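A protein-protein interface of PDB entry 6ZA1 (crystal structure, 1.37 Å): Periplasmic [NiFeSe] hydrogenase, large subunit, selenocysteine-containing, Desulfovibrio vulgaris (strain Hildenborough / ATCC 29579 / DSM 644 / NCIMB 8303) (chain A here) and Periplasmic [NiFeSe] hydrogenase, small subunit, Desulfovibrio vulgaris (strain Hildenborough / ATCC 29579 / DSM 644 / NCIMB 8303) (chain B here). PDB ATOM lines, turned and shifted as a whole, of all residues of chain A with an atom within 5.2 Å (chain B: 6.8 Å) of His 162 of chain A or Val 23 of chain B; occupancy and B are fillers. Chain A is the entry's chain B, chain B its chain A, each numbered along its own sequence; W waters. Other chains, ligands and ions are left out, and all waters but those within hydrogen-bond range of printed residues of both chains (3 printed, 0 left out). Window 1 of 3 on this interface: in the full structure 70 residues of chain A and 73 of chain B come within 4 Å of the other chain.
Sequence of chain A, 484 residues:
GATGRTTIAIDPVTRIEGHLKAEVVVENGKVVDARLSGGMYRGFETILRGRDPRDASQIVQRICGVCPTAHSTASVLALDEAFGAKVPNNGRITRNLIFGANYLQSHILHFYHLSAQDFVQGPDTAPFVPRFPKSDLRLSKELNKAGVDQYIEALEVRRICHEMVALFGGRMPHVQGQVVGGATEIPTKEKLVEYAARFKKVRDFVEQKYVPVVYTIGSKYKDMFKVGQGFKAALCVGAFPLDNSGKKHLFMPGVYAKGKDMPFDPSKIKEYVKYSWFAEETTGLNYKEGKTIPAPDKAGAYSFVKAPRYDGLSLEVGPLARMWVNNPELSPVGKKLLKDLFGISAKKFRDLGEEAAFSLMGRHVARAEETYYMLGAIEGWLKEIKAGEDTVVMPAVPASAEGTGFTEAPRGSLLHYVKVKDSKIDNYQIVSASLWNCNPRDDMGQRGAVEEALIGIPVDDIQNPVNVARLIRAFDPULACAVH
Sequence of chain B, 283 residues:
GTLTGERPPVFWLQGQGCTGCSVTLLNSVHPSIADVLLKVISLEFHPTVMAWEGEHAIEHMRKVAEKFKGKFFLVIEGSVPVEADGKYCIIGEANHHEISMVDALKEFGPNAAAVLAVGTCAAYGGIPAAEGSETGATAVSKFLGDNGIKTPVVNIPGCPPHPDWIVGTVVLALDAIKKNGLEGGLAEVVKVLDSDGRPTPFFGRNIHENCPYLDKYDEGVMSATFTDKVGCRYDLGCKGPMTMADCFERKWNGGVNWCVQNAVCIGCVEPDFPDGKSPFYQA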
ATOM      1  N   GLY A  65     -16.347  -5.134   1.200  1.00  0.00           N
ATOM      2  CA  GLY A  65     -15.490  -5.955   2.026  1.00  0.00           C
ATOM      3  C   GLY A  65     -15.459  -7.419   1.679  1.00  0.00           C
ATOM      4  O   GLY A  65     -14.728  -8.184   2.317  1.00  0.00           O
ATOM      5  N   VAL A  66     -16.247  -7.832   0.693  1.00  0.00           N
ATOM      6  CA  VAL A  66     -16.166  -9.188   0.160  1.00  0.00           C
ATOM      7  C   VAL A  66     -15.128  -9.270  -0.954  1.00  0.00           C
ATOM      8  O   VAL A  66     -14.370 -10.239  -1.025  1.00  0.00           O
ATOM      9  CB  VAL A  66     -17.550  -9.649  -0.334  1.00  0.00           C
ATOM     10  CG1 VAL A  66     -17.462 -11.053  -0.927  1.00  0.00           C
ATOM     11  CG2 VAL A  66     -18.573  -9.604   0.794  1.00  0.00           C
ATOM     12  N   ASN A 102      -8.217 -14.588  -2.725  1.00  0.00           N
ATOM     13  CA  ASN A 102      -9.577 -14.140  -2.454  1.00  0.00           C
ATOM     14  C   ASN A 102     -10.596 -14.636  -3.472  1.00  0.00           C
ATOM     15  O   ASN A 102     -11.786 -14.672  -3.151  1.00  0.00           O
ATOM     16  CB  ASN A 102      -9.719 -12.633  -2.336  1.00  0.00           C
ATOM     17  CG  ASN A 102     -10.948 -12.260  -1.528  1.00  0.00           C
ATOM     18  OD1 ASN A 102     -11.159 -12.795  -0.441  1.00  0.00           O
ATOM     19  ND2 ASN A 102     -11.795 -11.399  -2.076  1.00  0.00           N
ATOM     20  N   GLN A 105     -11.636 -17.604  -1.660  1.00  0.00           N
ATOM     21  CA  GLN A 105     -12.503 -17.239  -0.542  1.00  0.00           C
ATOM     22  C   GLN A 105     -13.896 -16.888  -1.024  1.00  0.00           C
ATOM     23  O   GLN A 105     -14.899 -17.336  -0.452  1.00  0.00           O
ATOM     24  CB  GLN A 105     -11.933 -16.038   0.213  1.00  0.00           C
ATOM     25  CG  GLN A 105     -12.748 -15.645   1.475  1.00  0.00           C
ATOM     26  CD  GLN A 105     -13.913 -14.660   1.253  1.00  0.00           C
ATOM     27  OE1 GLN A 105     -14.889 -14.683   2.008  1.00  0.00           O
ATOM     28  NE2 GLN A 105     -13.792 -13.766   0.272  1.00  0.00           N
ATOM     29  N   ARG A 158     -12.923 -20.931   4.060  1.00  0.00           N
ATOM     30  CA  ARG A 158     -12.871 -19.544   3.601  1.00  0.00           C
ATOM     31  C   ARG A 158     -12.008 -18.689   4.524  1.00  0.00           C
ATOM     32  O   ARG A 158     -11.333 -17.763   4.061  1.00  0.00           O
ATOM     33  CB  ARG A 158     -14.271 -18.943   3.412  1.00  0.00           C
ATOM     34  CG  ARG A 158     -15.113 -18.790   4.660  1.00  0.00           C
ATOM     35  CD  ARG A 158     -16.058 -17.586   4.563  1.00  0.00           C
ATOM     36  NE  ARG A 158     -15.316 -16.348   4.323  1.00  0.00           N
ATOM     37  CZ  ARG A 158     -14.490 -15.783   5.196  1.00  0.00           C
ATOM     38  NH1 ARG A 158     -14.289 -16.332   6.387  1.00  0.00           N
ATOM     39  NH2 ARG A 158     -13.855 -14.663   4.877  1.00  0.00           N
ATOM     40  N   ARG A 159     -12.001 -18.988   5.825  1.00  0.00           N
ATOM     41  CA  ARG A 159     -11.143 -18.247   6.745  1.00  0.00           C
ATOM     42  C   ARG A 159      -9.674 -18.494   6.431  1.00  0.00           C
ATOM     43  O   ARG A 159      -8.866 -17.555   6.435  1.00  0.00           O
ATOM     44  CB  ARG A 159     -11.479 -18.638   8.185  1.00  0.00           C
ATOM     45  CG  ARG A 159     -10.671 -17.912   9.237  1.00  0.00           C
ATOM     46  CD  ARG A 159     -10.959 -18.436  10.646  1.00  0.00           C
ATOM     47  NE  ARG A 159     -10.497 -19.810  10.846  1.00  0.00           N
ATOM     48  CZ  ARG A 159      -9.219 -20.160  10.951  1.00  0.00           C
ATOM     49  NH1 ARG A 159      -8.270 -19.237  10.861  1.00  0.00           N
ATOM     50  NH2 ARG A 159      -8.893 -21.435  11.137  1.00  0.00           N
ATOM     51  N   ILE A 160      -9.318 -19.746   6.141  1.00  0.00           N
ATOM     52  CA  ILE A 160      -7.952 -20.076   5.741  1.00  0.00           C
ATOM     53  C   ILE A 160      -7.562 -19.306   4.486  1.00  0.00           C
ATOM     54  O   ILE A 160      -6.417 -18.850   4.351  1.00  0.00           O
ATOM     55  CB  ILE A 160      -7.814 -21.605   5.574  1.00  0.00           C
ATOM     56  CG1 ILE A 160      -7.969 -22.296   6.936  1.00  0.00           C
ATOM     57  CG2 ILE A 160      -6.488 -21.953   4.921  1.00  0.00           C
ATOM     58  CD1 ILE A 160      -8.220 -23.799   6.868  1.00  0.00           C
ATOM     59  N   CYS A 161      -8.503 -19.123   3.557  1.00  0.00           N
ATOM     60  CA  CYS A 161      -8.205 -18.350   2.353  1.00  0.00           C
ATOM     61  C   CYS A 161      -7.832 -16.914   2.703  1.00  0.00           C
ATOM     62  O   CYS A 161      -6.941 -16.324   2.079  1.00  0.00           O
ATOM     63  CB  CYS A 161      -9.395 -18.365   1.393  1.00  0.00           C
ATOM     64  SG  CYS A 161      -9.786 -19.943   0.601  1.00  0.00           S
ATOM     65  N   HIS A 162      -8.515 -16.320   3.688  1.00  0.00           N
ATOM     66  CA  HIS A 162      -8.148 -14.969   4.106  1.00  0.00           C
ATOM     67  C   HIS A 162      -6.792 -14.940   4.797  1.00  0.00           C
ATOM     68  O   HIS A 162      -6.058 -13.951   4.655  1.00  0.00           O
ATOM     69  CB  HIS A 162      -9.271 -14.329   4.923  1.00  0.00           C
ATOM     70  CG  HIS A 162     -10.246 -13.582   4.067  1.00  0.00           C
ATOM     71  ND1 HIS A 162     -11.267 -12.803   4.572  1.00  0.00           N
ATOM     72  CD2 HIS A 162     -10.340 -13.488   2.718  1.00  0.00           C
ATOM     73  CE1 HIS A 162     -11.951 -12.272   3.570  1.00  0.00           C
ATOM     74  NE2 HIS A 162     -11.402 -12.672   2.437  1.00  0.00           N
ATOM     75  N   GLU A 163      -6.413 -15.999   5.516  1.00  0.00           N
ATOM     76  CA  GLU A 163      -5.044 -16.071   6.022  1.00  0.00           C
ATOM     77  C   GLU A 163      -4.053 -16.065   4.865  1.00  0.00           C
ATOM     78  O   GLU A 163      -3.001 -15.416   4.942  1.00  0.00           O
ATOM     79  CB  GLU A 163      -4.848 -17.306   6.900  1.00  0.00           C
ATOM     80  CG  GLU A 163      -5.729 -17.307   8.137  1.00  0.00           C
ATOM     81  CD  GLU A 163      -5.394 -18.425   9.106  1.00  0.00           C
ATOM     82  OE1 GLU A 163      -4.713 -19.383   8.693  1.00  0.00           O
ATOM     83  OE2 GLU A 163      -5.810 -18.334  10.280  1.00  0.00           O
ATOM     84  N   MET A 164      -4.379 -16.764   3.780  1.00  0.00           N
ATOM     85  CA  MET A 164      -3.512 -16.737   2.602  1.00  0.00           C
ATOM     86  C   MET A 164      -3.395 -15.322   2.049  1.00  0.00           C
ATOM     87  O   MET A 164      -2.292 -14.859   1.737  1.00  0.00           O
ATOM     88  CB  MET A 164      -4.036 -17.695   1.535  1.00  0.00           C
ATOM     89  CG  MET A 164      -3.867 -19.154   1.907  1.00  0.00           C
ATOM     90  SD  MET A 164      -4.888 -20.257   0.917  1.00  0.00           S
ATOM     91  CE  MET A 164      -4.293 -19.903  -0.735  1.00  0.00           C
ATOM     92  N   VAL A 165      -4.525 -14.621   1.922  1.00  0.00           N
ATOM     93  CA  VAL A 165      -4.493 -13.236   1.455  1.00  0.00           C
ATOM     94  C   VAL A 165      -3.602 -12.392   2.358  1.00  0.00           C
ATOM     95  O   VAL A 165      -2.788 -11.588   1.886  1.00  0.00           O
ATOM     96  CB  VAL A 165      -5.915 -12.647   1.406  1.00  0.00           C
ATOM     97  CG1 VAL A 165      -5.855 -11.145   1.097  1.00  0.00           C
ATOM     98  CG2 VAL A 165      -6.777 -13.375   0.403  1.00  0.00           C
ATOM     99  N   ALA A 166      -3.772 -12.538   3.670  1.00  0.00           N
ATOM    100  CA  ALA A 166      -3.096 -11.658   4.613  1.00  0.00           C
ATOM    101  C   ALA A 166      -1.601 -11.938   4.726  1.00  0.00           C
ATOM    102  O   ALA A 166      -0.856 -11.045   5.131  1.00  0.00           O
ATOM    103  CB  ALA A 166      -3.757 -11.775   5.987  1.00  0.00           C
ATOM    104  N   LEU A 167      -1.142 -13.141   4.379  1.00  0.00           N
ATOM    105  CA  LEU A 167       0.286 -13.443   4.496  1.00  0.00           C
ATOM    106  C   LEU A 167       1.145 -12.406   3.773  1.00  0.00           C
ATOM    107  O   LEU A 167       2.168 -11.958   4.302  1.00  0.00           O
ATOM    108  CB  LEU A 167       0.562 -14.855   3.985  1.00  0.00           C
ATOM    109  CG  LEU A 167       0.363 -15.928   5.061  1.00  0.00           C
ATOM    110  CD1 LEU A 167       0.219 -17.304   4.441  1.00  0.00           C
ATOM    111  CD2 LEU A 167       1.516 -15.897   6.065  1.00  0.00           C
ATOM    112  N   MET A 172      -7.081  -8.878   5.993  1.00  0.00           N
ATOM    113  CA  MET A 172      -8.210  -9.018   5.080  1.00  0.00           C
ATOM    114  C   MET A 172      -9.449  -9.147   5.949  1.00  0.00           C
ATOM    115  O   MET A 172      -9.425  -9.885   6.940  1.00  0.00           O
ATOM    116  CB  MET A 172      -8.035 -10.272   4.228  1.00  0.00           C
ATOM    117  CG  MET A 172      -9.031 -10.383   3.097  1.00  0.00           C
ATOM    118  SD  MET A 172      -8.870  -9.089   1.856  1.00  0.00           S
ATOM    119  CE  MET A 172      -9.883  -9.825   0.577  1.00  0.00           C
ATOM    120  N   PRO A 173     -10.547  -8.441   5.644  1.00  0.00           N
ATOM    121  CA  PRO A 173     -10.720  -7.474   4.552  1.00  0.00           C
ATOM    122  C   PRO A 173      -9.789  -6.258   4.584  1.00  0.00           C
ATOM    123  O   PRO A 173      -9.299  -5.864   5.648  1.00  0.00           O
ATOM    124  CB  PRO A 173     -12.169  -6.988   4.735  1.00  0.00           C
ATOM    125  CG  PRO A 173     -12.859  -8.085   5.459  1.00  0.00           C
ATOM    126  CD  PRO A 173     -11.810  -8.680   6.370  1.00  0.00           C
ATOM    127  N   TRP B  12     -28.995  -7.696  12.826  1.00  0.00           N
ATOM    128  CA  TRP B  12     -27.836  -7.059  12.206  1.00  0.00           C
ATOM    129  C   TRP B  12     -28.370  -6.245  11.040  1.00  0.00           C
ATOM    130  O   TRP B  12     -28.809  -6.812  10.032  1.00  0.00           O
ATOM    131  CB  TRP B  12     -26.864  -8.136  11.723  1.00  0.00           C
ATOM    132  CG  TRP B  12     -25.523  -7.641  11.254  1.00  0.00           C
ATOM    133  CD1 TRP B  12     -25.271  -6.850  10.172  1.00  0.00           C
ATOM    134  CD2 TRP B  12     -24.245  -7.943  11.836  1.00  0.00           C
ATOM    135  NE1 TRP B  12     -23.917  -6.630  10.051  1.00  0.00           N
ATOM    136  CE2 TRP B  12     -23.267  -7.290  11.058  1.00  0.00           C
ATOM    137  CE3 TRP B  12     -23.834  -8.695  12.942  1.00  0.00           C
ATOM    138  CZ2 TRP B  12     -21.906  -7.364  11.353  1.00  0.00           C
ATOM    139  CZ3 TRP B  12     -22.486  -8.768  13.231  1.00  0.00           C
ATOM    140  CH2 TRP B  12     -21.537  -8.109  12.437  1.00  0.00           C
ATOM    141  N   CYS B  18     -19.960  -1.767   3.797  1.00  0.00           N
ATOM    142  CA  CYS B  18     -19.396  -2.549   2.711  1.00  0.00           C
ATOM    143  C   CYS B  18     -19.422  -4.045   2.994  1.00  0.00           C
ATOM    144  O   CYS B  18     -18.886  -4.817   2.193  1.00  0.00           O
ATOM    145  CB  CYS B  18     -17.962  -2.083   2.398  1.00  0.00           C
ATOM    146  SG  CYS B  18     -16.621  -2.755   3.426  1.00  0.00           S
ATOM    147  N   THR B  19     -20.045  -4.470   4.102  1.00  0.00           N
ATOM    148  CA  THR B  19     -20.172  -5.872   4.524  1.00  0.00           C
ATOM    149  C   THR B  19     -18.830  -6.352   5.067  1.00  0.00           C
ATOM    150  O   THR B  19     -18.708  -7.523   5.469  1.00  0.00           O
ATOM    151  CB  THR B  19     -20.768  -6.745   3.413  1.00  0.00           C
ATOM    152  OG1 THR B  19     -22.008  -6.145   2.994  1.00  0.00           O
ATOM    153  CG2 THR B  19     -21.068  -8.131   3.903  1.00  0.00           C
ATOM    154  N   GLY B  20     -17.837  -5.457   5.172  1.00  0.00           N
ATOM    155  CA  GLY B  20     -16.556  -5.831   5.745  1.00  0.00           C
ATOM    156  C   GLY B  20     -16.645  -6.245   7.198  1.00  0.00           C
ATOM    157  O   GLY B  20     -15.851  -7.069   7.660  1.00  0.00           O
ATOM    158  N   CYS B  21     -17.600  -5.670   7.942  1.00  0.00           N
ATOM    159  CA  CYS B  21     -17.800  -6.072   9.332  1.00  0.00           C
ATOM    160  C   CYS B  21     -18.277  -7.512   9.407  1.00  0.00           C
ATOM    161  O   CYS B  21     -17.796  -8.306  10.222  1.00  0.00           O
ATOM    162  CB  CYS B  21     -18.831  -5.163  10.011  1.00  0.00           C
ATOM    163  SG  CYS B  21     -18.215  -3.640  10.747  1.00  0.00           S
ATOM    164  N   SER B  22     -19.248  -7.869   8.573  1.00  0.00           N
ATOM    165  CA  SER B  22     -19.706  -9.255   8.570  1.00  0.00           C
ATOM    166  C   SER B  22     -18.572 -10.198   8.177  1.00  0.00           C
ATOM    167  O   SER B  22     -18.364 -11.241   8.811  1.00  0.00           O
ATOM    168  CB  SER B  22     -20.886  -9.434   7.617  1.00  0.00           C
ATOM    169  OG  SER B  22     -22.059  -8.874   8.164  1.00  0.00           O
ATOM    170  N   VAL B  23     -17.824  -9.849   7.127  1.00  0.00           N
ATOM    171  CA  VAL B  23     -16.747 -10.721   6.665  1.00  0.00           C
ATOM    172  C   VAL B  23     -15.679 -10.889   7.740  1.00  0.00           C
ATOM    173  O   VAL B  23     -15.191 -11.999   7.975  1.00  0.00           O
ATOM    174  CB  VAL B  23     -16.158 -10.212   5.337  1.00  0.00           C
ATOM    175  CG1 VAL B  23     -14.946 -11.041   4.934  1.00  0.00           C
ATOM    176  CG2 VAL B  23     -17.226 -10.241   4.252  1.00  0.00           C
ATOM    177  N   THR B  24     -15.282  -9.794   8.392  1.00  0.00           N
ATOM    178  CA  THR B  24     -14.264  -9.915   9.435  1.00  0.00           C
ATOM    179  C   THR B  24     -14.733 -10.847  10.546  1.00  0.00           C
ATOM    180  O   THR B  24     -13.963 -11.678  11.040  1.00  0.00           O
ATOM    181  CB  THR B  24     -13.848  -8.526   9.940  1.00  0.00           C
ATOM    182  OG1 THR B  24     -12.507  -8.608  10.451  1.00  0.00           O
ATOM    183  CG2 THR B  24     -14.780  -7.990  11.009  1.00  0.00           C
ATOM    184  N   LEU B  25     -16.016 -10.766  10.904  1.00  0.00           N
ATOM    185  CA  LEU B  25     -16.566 -11.661  11.914  1.00  0.00           C
ATOM    186  C   LEU B  25     -16.489 -13.116  11.472  1.00  0.00           C
ATOM    187  O   LEU B  25     -16.187 -13.998  12.283  1.00  0.00           O
ATOM    188  CB  LEU B  25     -18.003 -11.248  12.212  1.00  0.00           C
ATOM    189  CG  LEU B  25     -18.734 -12.124  13.228  1.00  0.00           C
ATOM    190  CD1 LEU B  25     -18.013 -12.117  14.559  1.00  0.00           C
ATOM    191  CD2 LEU B  25     -20.174 -11.650  13.354  1.00  0.00           C
ATOM    192  N   LEU B  26     -16.741 -13.389  10.188  1.00  0.00           N
ATOM    193  CA  LEU B  26     -16.602 -14.747   9.682  1.00  0.00           C
ATOM    194  C   LEU B  26     -15.190 -15.294   9.867  1.00  0.00           C
ATOM    195  O   LEU B  26     -14.997 -16.513   9.823  1.00  0.00           O
ATOM    196  CB  LEU B  26     -16.957 -14.801   8.195  1.00  0.00           C
ATOM    197  CG  LEU B  26     -18.372 -14.396   7.794  1.00  0.00           C
ATOM    198  CD1 LEU B  26     -18.568 -14.471   6.292  1.00  0.00           C
ATOM    199  CD2 LEU B  26     -19.386 -15.282   8.484  1.00  0.00           C
ATOM    200  N   ASN B  27     -14.198 -14.430  10.070  1.00  0.00           N
ATOM    201  CA  ASN B  27     -12.823 -14.863  10.237  1.00  0.00           C
ATOM    202  C   ASN B  27     -12.447 -15.146  11.690  1.00  0.00           C
ATOM    203  O   ASN B  27     -11.281 -15.413  11.971  1.00  0.00           O
ATOM    204  CB  ASN B  27     -11.856 -13.824   9.659  1.00  0.00           C
ATOM    205  CG  ASN B  27     -11.871 -13.788   8.145  1.00  0.00           C
ATOM    206  OD1 ASN B  27     -12.252 -14.758   7.491  1.00  0.00           O
ATOM    207  ND2 ASN B  27     -11.456 -12.660   7.585  1.00  0.00           N
ATOM    208  N   SER B  28     -13.408 -15.101  12.615  1.00  0.00           N
ATOM    209  CA  SER B  28     -13.099 -15.392  14.012  1.00  0.00           C
ATOM    210  C   SER B  28     -12.519 -16.792  14.150  1.00  0.00           C
ATOM    211  O   SER B  28     -13.042 -17.759  13.590  1.00  0.00           O
ATOM    212  CB  SER B  28     -14.372 -15.270  14.846  1.00  0.00           C
ATOM    213  OG  SER B  28     -14.081 -15.397  16.226  1.00  0.00           O
ATOM    214  N   THR B  48     -27.231 -10.807   4.839  1.00  0.00           N
ATOM    215  CA  THR B  48     -26.230 -11.500   4.042  1.00  0.00           C
ATOM    216  C   THR B  48     -26.316 -13.013   4.187  1.00  0.00           C
ATOM    217  O   THR B  48     -25.915 -13.733   3.268  1.00  0.00           O
ATOM    218  CB  THR B  48     -24.823 -11.025   4.410  1.00  0.00           C
ATOM    219  OG1 THR B  48     -24.817  -9.594   4.502  1.00  0.00           O
ATOM    220  CG2 THR B  48     -23.800 -11.484   3.361  1.00  0.00           C
ATOM    221  N   PRO B 160     -11.829  -2.935   8.493  1.00  0.00           N
ATOM    222  CA  PRO B 160     -12.840  -3.357   9.465  1.00  0.00           C
ATOM    223  C   PRO B 160     -12.272  -3.555  10.865  1.00  0.00           C
ATOM    224  O   PRO B 160     -11.054  -3.504  11.047  1.00  0.00           O
ATOM    225  CB  PRO B 160     -13.267  -4.722   8.922  1.00  0.00           C
ATOM    226  CG  PRO B 160     -11.979  -5.282   8.393  1.00  0.00           C
ATOM    227  CD  PRO B 160     -11.204  -4.093   7.826  1.00  0.00           C
ATOM    228  N   PRO B 163     -11.967  -9.406  14.194  1.00  0.00           N
ATOM    229  CA  PRO B 163     -13.082 -10.204  14.724  1.00  0.00           C
ATOM    230  C   PRO B 163     -13.067 -10.314  16.232  1.00  0.00           C
ATOM    231  O   PRO B 163     -14.140 -10.353  16.856  1.00  0.00           O
ATOM    232  CB  PRO B 163     -12.906 -11.578  14.055  1.00  0.00           C
ATOM    233  CG  PRO B 163     -11.498 -11.612  13.594  1.00  0.00           C
ATOM    234  CD  PRO B 163     -11.155 -10.176  13.234  1.00  0.00           C
ATOM    235  N   ASN B 253      -5.842 -12.023  11.029  1.00  0.00           N
ATOM    236  CA  ASN B 253      -6.068 -13.223  10.239  1.00  0.00           C
ATOM    237  C   ASN B 253      -5.252 -14.402  10.761  1.00  0.00           C
ATOM    238  O   ASN B 253      -4.449 -15.016  10.056  1.00  0.00           O
ATOM    239  CB  ASN B 253      -5.798 -12.952   8.757  1.00  0.00           C
ATOM    240  CG  ASN B 253      -6.681 -11.857   8.205  1.00  0.00           C
ATOM    241  OD1 ASN B 253      -6.285 -10.692   8.141  1.00  0.00           O
ATOM    242  ND2 ASN B 253      -7.894 -12.221   7.815  1.00  0.00           N
ATOM    243  N   VAL B 256      -1.109 -14.035  11.117  1.00  0.00           N
ATOM    244  CA  VAL B 256      -0.151 -14.171  10.021  1.00  0.00           C
ATOM    245  C   VAL B 256       0.512 -12.847   9.649  1.00  0.00           C
ATOM    246  O   VAL B 256       1.564 -12.858   8.989  1.00  0.00           O
ATOM    247  CB  VAL B 256      -0.744 -14.816   8.755  1.00  0.00           C
ATOM    248  CG1 VAL B 256      -1.271 -16.209   9.067  1.00  0.00           C
ATOM    249  CG2 VAL B 256      -1.832 -13.952   8.140  1.00  0.00           C
HETATM  250  O   HOH W   1      -8.619 -15.062   8.206  1.00  0.00           O
HETATM  251  O   HOH W   2     -15.913 -18.237   7.848  1.00  0.00           O
HETATM  252  O   HOH W   3     -10.602 -10.414   9.460  1.00  0.00           O
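OE2 of Glu 163 of chain A lies within salt-bridge range of NH1 of Arg 159 of chain A (2.7 Å).
NH2 of Arg 158 of chain A is in hydrogen-bond range of ND1 of His 162 of chain A, at 3.2 Å.
NE2 of Gln 105 of chain A lies close to NE2 of His 162 of chain A, at 3.4 Å.
NE2 of His 162 of chain A lies within hydrogen-bond range of OD1 of Asn 102 of chain A, 2.9 Å away.
The guanidinium group (NE) of Arg 158 of chain A lies within hydrogen-bond range of the side-chain amide oxygen (OE1) of Gln 105 of chain A (2.9 Å).
The side-chain sulfur (SG) of Cys 18 of chain B sits close to the backbone NH (N) of Gly 20 of chain B (3.4 Å).
The side-chain amide nitrogen (ND2) of Asn 27 of chain B sits at hydrogen-bond distance from the backbone carbonyl oxygen (O) of Met 172 of chain A (3.5 Å).
O of Cys 18 of chain B lies within hydrogen-bond range of N of Gly 65 of chain A, at 2.7 Å.
The side-chain amide oxygen of Asn 27 of chain B sits at hydrogen-bond distance from the guanidinium group of Arg 158 of chain A (2.8 Å).
OD1 of Asn 253 of chain B sits at hydrogen-bond distance from N of Met 172 of chain A, at 2.9 Å.
ND2 of Asn 27 of chain B lies within hydrogen-bond range of ND1 of His 162 of chain A (3.0 Å).
Of the printed residues of chain B, Val 66 of chain A touches Val 23.
Gln 105 of chain A touches none of the printed residues of chain B.
Of the printed residues of chain B, Arg 159 of chain A touches Asn 27 (3.3 Å) and Ser 28 (3.7 Å).
His 162 of chain A touches three residues of chain B.
Printed residues of chain B within 4 Å of Leu 167 of chain A: Val 256 (3.7 Å).
Printed residues of chain A within 4 Å of Cys 18 of chain B: Gly 65.
Val 23 of chain B touches just these residues of chain A: Gly 65, Val 66, Arg 158, His 162 and Pro 173.
Leu 25 of chain B touches none of the printed residues of chain A.
Of the 17 printed residues of chain B, 9 touch a printed residue of chain A.
Hydrophobic or aromatic side chains of chain B within 4 Å of the printed part of chain A: Val 23, Leu 26, Pro 160 and Val 256.
Of the 16 printed residues of chain A, 10 touch a printed residue of chain B.
Printed residues of chain A that touch a printed residue of chain B: Gly 65, Val 66, Arg 158, Arg 159, His 162, Glu 163, Ala 166, Leu 167, Met 172 and Pro 173.
Hydrophobic or aromatic side chains of chain A within 4 Å of the printed part of chain B: Val 66, His 162, Ala 166, Leu 167 and Pro 173.
Water W2 lies within hydrogen-bond range of O of Leu 26 of chain B (2.8 Å) and NH1 of Arg 158 of chain A (2.9 Å).
Water W3 lies within hydrogen-bond range of OG1 of Thr 24 of chain B (2.8 Å), O of Met 172 of chain A (2.8 Å) and ND2 of Asn 27 of chain B (3.0 Å).
Water W1 lies within hydrogen-bond range of the side-chain amide nitrogen (ND2) of Asn 253 of chain B (3.0 Å) and the backbone carbonyl oxygen (O) of Arg 159 of chain A (3.1 Å).
Among the printed residues, pairs that only touch across the chains: Gly 65 of chain A with Gly 20 of chain B, Gly 65 of chain A with Val 23 of chain B, Val 66 of chain A with Val 23 of chain B, Arg 158 of chain A with Val 23 of chain B, Arg 158 of chain A with Leu 26 of chain B, Arg 159 of chain A with Asn 27 of chain B, Arg 159 of chain A with Ser 28 of chain B, His 162 of chain A with Val 23 of chain B, His 162 of chain A with Asn 253 of chain B, Glu 163 of chain A with Asn 253 of chain B, Glu 163 of chain A with Val 256 of chain B, Ala 166 of chain A with Asn 253 of chain B, Ala 166 of chain A with Val 256 of chain B, Leu 167 of chain A with Val 256 of chain B, Pro 173 of chain A with Gly 20 of chain B, Pro 173 of chain A with Val 23 of chain B and Pro 173 of chain A with Pro 160 of chain B.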
